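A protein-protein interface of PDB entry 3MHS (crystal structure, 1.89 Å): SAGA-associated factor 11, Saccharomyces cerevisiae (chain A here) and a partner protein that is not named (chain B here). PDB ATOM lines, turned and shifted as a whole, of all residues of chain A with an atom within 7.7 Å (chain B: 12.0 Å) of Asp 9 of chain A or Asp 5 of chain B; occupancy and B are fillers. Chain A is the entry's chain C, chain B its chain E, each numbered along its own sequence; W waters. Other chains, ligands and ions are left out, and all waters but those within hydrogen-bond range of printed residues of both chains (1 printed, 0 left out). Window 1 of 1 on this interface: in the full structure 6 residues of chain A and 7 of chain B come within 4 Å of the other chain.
The backbone NH (N) of Ile 8 of chain B lies close to the backbone carbonyl oxygen (O) of Ile 6 of chain A.
OG of Ser 10 of chain A is in hydrogen-bond range of N of Thr 7 of chain A (2.8 Å).
Among the printed residues, merely in contact across the chains: Thr 5 of chain A with Glu 7 of chain B, Thr 7 of chain A with Ala 6 of chain B, Asp 9 of chain A with Asp 5 of chain B, Ile 6 of chain A with Glu 7 of chain B and Thr 7 of chain A with Ile 8 of chain B.
Of the printed residues of chain B, Ile 6 of chain A touches Glu 7 (3.7 Å) and Ile 8 (2.9 Å).
Of chain B, only Ala 6 and Ile 8 come within 4 Å of Thr 7 of chain A.
Ile 8 of chain A touches none of the printed residues of chain B.
Asp 9 of chain A touches one residue of chain B.
No residue of chain B comes within 4 Å of Ser 10 of chain A.
Ser 12 of chain A touches none of the printed residues of chain B.
No residue of chain B comes within 4 Å of Asn 13 of chain A.
Of chain A, only Asp 9 comes within 4 Å of Asp 5 of chain B.
Printed residues of chain A within 4 Å of Ala 6 of chain B: Thr 7 (3.4 Å).
Of the printed residues of chain A, Glu 7 of chain B touches Thr 5 and Ile 6.
Lys 9 of chain B touches none of the printed residues of chain A.
The nearest residue of chain A that does not touch Asp 5 of chain B is Ile 8 of chain A (4.7 Å).
Of the 5 printed residues of chain B, 4 touch a printed residue of chain A.
Hydrophobic or aromatic side chains of chain B that line the printed part of chain A: Ile 8.
Printed residues of chain A that touch a printed residue of chain B: Thr 5, Ile 6, Thr 7 and Asp 9.
Hydrophobic or aromatic side chains of chain A that line the printed part of chain B: Ile 6.
Among the printed residues, 6 pairs touch across the chains.
Water W1 lies within hydrogen-bond range of the backbone carbonyl oxygen (O) of Ala 6 of chain B (2.7 Å), the backbone NH (N) of Asp 5 of chain B (3.0 Å) and the backbone NH (N) of Ile 8 of chain A (3.0 Å).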
ATOM      1  N   THR A   5     -25.122 -20.510   5.333  1.00  0.00           N
ATOM      2  CA  THR A   5     -24.515 -21.562   4.522  1.00  0.00           C
ATOM      3  C   THR A   5     -25.251 -22.893   4.682  1.00  0.00           C
ATOM      4  O   THR A   5     -25.670 -23.253   5.785  1.00  0.00           O
ATOM      5  CB  THR A   5     -23.038 -21.777   4.925  1.00  0.00           C
ATOM      6  OG1 THR A   5     -22.366 -20.510   5.000  1.00  0.00           O
ATOM      7  CG2 THR A   5     -22.333 -22.681   3.922  1.00  0.00           C
ATOM      8  N   ILE A   6     -25.394 -23.617   3.576  1.00  0.00           N
ATOM      9  CA  ILE A   6     -26.066 -24.904   3.601  1.00  0.00           C
ATOM     10  C   ILE A   6     -25.042 -26.025   3.436  1.00  0.00           C
ATOM     11  O   ILE A   6     -24.203 -26.001   2.525  1.00  0.00           O
ATOM     12  CB  ILE A   6     -27.205 -24.992   2.544  1.00  0.00           C
ATOM     13  CG1 ILE A   6     -26.641 -25.096   1.115  1.00  0.00           C
ATOM     14  CG2 ILE A   6     -28.124 -23.761   2.663  1.00  0.00           C
ATOM     15  CD1 ILE A   6     -27.480 -25.986   0.184  1.00  0.00           C
ATOM     16  N   THR A   7     -25.118 -26.989   4.350  1.00  0.00           N
ATOM     17  CA  THR A   7     -24.177 -28.094   4.422  1.00  0.00           C
ATOM     18  C   THR A   7     -24.953 -29.398   4.661  1.00  0.00           C
ATOM     19  O   THR A   7     -26.066 -29.380   5.195  1.00  0.00           O
ATOM     20  CB  THR A   7     -23.214 -27.895   5.620  1.00  0.00           C
ATOM     21  OG1 THR A   7     -23.969 -27.850   6.846  1.00  0.00           O
ATOM     22  CG2 THR A   7     -22.419 -26.603   5.470  1.00  0.00           C
ATOM     23  N   ILE A   8     -24.349 -30.523   4.282  1.00  0.00           N
ATOM     24  CA  ILE A   8     -24.892 -31.834   4.621  1.00  0.00           C
ATOM     25  C   ILE A   8     -25.302 -31.832   6.103  1.00  0.00           C
ATOM     26  O   ILE A   8     -26.416 -32.225   6.431  1.00  0.00           O
ATOM     27  CB  ILE A   8     -23.885 -32.970   4.321  1.00  0.00           C
ATOM     28  CG1 ILE A   8     -23.491 -32.982   2.834  1.00  0.00           C
ATOM     29  CG2 ILE A   8     -24.471 -34.341   4.673  1.00  0.00           C
ATOM     30  CD1 ILE A   8     -24.520 -33.586   1.911  1.00  0.00           C
ATOM     31  N   ASP A   9     -24.433 -31.359   6.995  1.00  0.00           N
ATOM     32  CA  ASP A   9     -24.793 -31.271   8.417  1.00  0.00           C
ATOM     33  C   ASP A   9     -26.064 -30.431   8.684  1.00  0.00           C
ATOM     34  O   ASP A   9     -26.933 -30.837   9.480  1.00  0.00           O
ATOM     35  CB  ASP A   9     -23.623 -30.743   9.246  1.00  0.00           C
ATOM     36  CG  ASP A   9     -22.588 -31.815   9.557  1.00  0.00           C
ATOM     37  OD1 ASP A   9     -22.556 -32.856   8.866  1.00  0.00           O
ATOM     38  OD2 ASP A   9     -21.794 -31.606  10.500  1.00  0.00           O
ATOM     39  N   SER A  10     -26.176 -29.269   8.033  1.00  0.00           N
ATOM     40  CA  SER A  10     -27.333 -28.378   8.227  1.00  0.00           C
ATOM     41  C   SER A  10     -28.609 -28.987   7.650  1.00  0.00           C
ATOM     42  O   SER A  10     -29.633 -29.045   8.338  1.00  0.00           O
ATOM     43  CB  SER A  10     -27.092 -26.974   7.628  1.00  0.00           C
ATOM     44  OG  SER A  10     -27.209 -26.955   6.209  1.00  0.00           O
ATOM     45  N   ILE A  11     -28.549 -29.436   6.400  1.00  0.00           N
ATOM     46  CA  ILE A  11     -29.719 -30.039   5.770  1.00  0.00           C
ATOM     47  C   ILE A  11     -30.153 -31.313   6.502  1.00  0.00           C
ATOM     48  O   ILE A  11     -31.338 -31.573   6.648  1.00  0.00           O
ATOM     49  CB  ILE A  11     -29.483 -30.395   4.298  1.00  0.00           C
ATOM     50  CG1 ILE A  11     -29.621 -29.158   3.420  1.00  0.00           C
ATOM     51  CG2 ILE A  11     -30.511 -31.419   3.862  1.00  0.00           C
ATOM     52  CD1 ILE A  11     -29.505 -29.455   1.943  1.00  0.00           C
ATOM     53  N   SER A  12     -29.184 -32.091   6.963  1.00  0.00           N
ATOM     54  CA  SER A  12     -29.462 -33.322   7.684  1.00  0.00           C
ATOM     55  C   SER A  12     -30.150 -33.012   9.001  1.00  0.00           C
ATOM     56  O   SER A  12     -31.097 -33.703   9.385  1.00  0.00           O
ATOM     57  CB  SER A  12     -28.170 -34.073   7.933  1.00  0.00           C
ATOM     58  OG  SER A  12     -27.651 -34.503   6.703  1.00  0.00           O
ATOM     59  N   ASN A  13     -29.684 -31.959   9.672  1.00  0.00           N
ATOM     60  CA  ASN A  13     -30.282 -31.514  10.926  1.00  0.00           C
ATOM     61  C   ASN A  13     -31.726 -31.097  10.675  1.00  0.00           C
ATOM     62  O   ASN A  13     -32.590 -31.305  11.523  1.00  0.00           O
ATOM     63  CB  ASN A  13     -29.501 -30.344  11.550  1.00  0.00           C
ATOM     64  CG  ASN A  13     -28.118 -30.753  12.063  1.00  0.00           C
ATOM     65  OD1 ASN A  13     -27.987 -31.657  12.888  1.00  0.00           O
ATOM     66  ND2 ASN A  13     -27.081 -30.048  11.598  1.00  0.00           N
ATOM     67  N   GLY A  14     -31.972 -30.504   9.506  1.00  0.00           N
ATOM     68  CA  GLY A  14     -33.304 -30.050   9.131  1.00  0.00           C
ATOM     69  C   GLY A  14     -34.216 -31.231   8.828  1.00  0.00           C
ATOM     70  O   GLY A  14     -35.399 -31.206   9.134  1.00  0.00           O
ATOM     71  N   ILE A  15     -33.662 -32.257   8.199  1.00  0.00           N
ATOM     72  CA  ILE A  15     -34.426 -33.462   7.918  1.00  0.00           C
ATOM     73  C   ILE A  15     -34.796 -34.117   9.231  1.00  0.00           C
ATOM     74  O   ILE A  15     -35.951 -34.434   9.436  1.00  0.00           O
ATOM     75  CB  ILE A  15     -33.674 -34.401   6.969  1.00  0.00           C
ATOM     76  CG1 ILE A  15     -33.736 -33.812   5.552  1.00  0.00           C
ATOM     77  CG2 ILE A  15     -34.281 -35.850   7.040  1.00  0.00           C
ATOM     78  CD1 ILE A  15     -32.745 -34.410   4.544  1.00  0.00           C
ATOM     79  N   ASP B   5     -20.057 -31.688   6.682  1.00  0.00           N
ATOM     80  CA  ASP B   5     -19.092 -30.725   7.290  1.00  0.00           C
ATOM     81  C   ASP B   5     -18.686 -29.603   6.317  1.00  0.00           C
ATOM     82  O   ASP B   5     -18.310 -28.510   6.752  1.00  0.00           O
ATOM     83  CB  ASP B   5     -17.849 -31.467   7.800  1.00  0.00           C
ATOM     84  CG  ASP B   5     -16.818 -31.723   6.705  1.00  0.00           C
ATOM     85  OD1 ASP B   5     -15.608 -31.584   6.992  1.00  0.00           O
ATOM     86  OD2 ASP B   5     -17.211 -32.050   5.561  1.00  0.00           O
ATOM     87  N   ALA B   6     -18.749 -29.878   5.010  1.00  0.00           N
ATOM     88  CA  ALA B   6     -18.405 -28.883   3.983  1.00  0.00           C
ATOM     89  C   ALA B   6     -19.658 -28.394   3.252  1.00  0.00           C
ATOM     90  O   ALA B   6     -20.765 -28.884   3.499  1.00  0.00           O
ATOM     91  CB  ALA B   6     -17.400 -29.461   2.987  1.00  0.00           C
ATOM     92  N   GLU B   7     -19.465 -27.455   2.326  1.00  0.00           N
ATOM     93  CA  GLU B   7     -20.577 -26.723   1.705  1.00  0.00           C
ATOM     94  C   GLU B   7     -21.155 -27.391   0.445  1.00  0.00           C
ATOM     95  O   GLU B   7     -20.428 -27.761  -0.481  1.00  0.00           O
ATOM     96  CB  GLU B   7     -20.130 -25.296   1.392  1.00  0.00           C
ATOM     97  CG  GLU B   7     -21.254 -24.285   1.227  1.00  0.00           C
ATOM     98  CD  GLU B   7     -20.736 -22.851   1.208  1.00  0.00           C
ATOM     99  OE1 GLU B   7     -21.520 -21.926   0.911  1.00  0.00           O
ATOM    100  OE2 GLU B   7     -19.539 -22.645   1.497  1.00  0.00           O
ATOM    101  N   ILE B   8     -22.479 -27.510   0.418  1.00  0.00           N
ATOM    102  CA  ILE B   8     -23.190 -28.191  -0.663  1.00  0.00           C
ATOM    103  C   ILE B   8     -23.487 -27.229  -1.807  1.00  0.00           C
ATOM    104  O   ILE B   8     -23.839 -26.076  -1.579  1.00  0.00           O
ATOM    105  CB  ILE B   8     -24.502 -28.831  -0.144  1.00  0.00           C
ATOM    106  CG1 ILE B   8     -25.326 -29.423  -1.291  1.00  0.00           C
ATOM    107  CG2 ILE B   8     -25.327 -27.811   0.625  1.00  0.00           C
ATOM    108  CD1 ILE B   8     -26.397 -30.385  -0.811  1.00  0.00           C
ATOM    109  N   LYS B   9     -23.350 -27.715  -3.035  1.00  0.00           N
ATOM    110  CA  LYS B   9     -23.458 -26.853  -4.210  1.00  0.00           C
ATOM    111  C   LYS B   9     -24.729 -27.085  -5.013  1.00  0.00           C
ATOM    112  O   LYS B   9     -25.354 -26.133  -5.483  1.00  0.00           O
ATOM    113  CB  LYS B   9     -22.225 -27.015  -5.109  1.00  0.00           C
ATOM    114  CG  LYS B   9     -21.042 -26.155  -4.672  1.00  0.00           C
ATOM    115  CD  LYS B   9     -21.263 -24.678  -5.010  1.00  0.00           C
ATOM    116  CE  LYS B   9     -21.006 -23.755  -3.810  1.00  0.00           C
ATOM    117  NZ  LYS B   9     -19.634 -23.876  -3.236  1.00  0.00           N
HETATM  118  O   HOH W   1     -21.486 -31.440   4.102  1.00  0.00           O
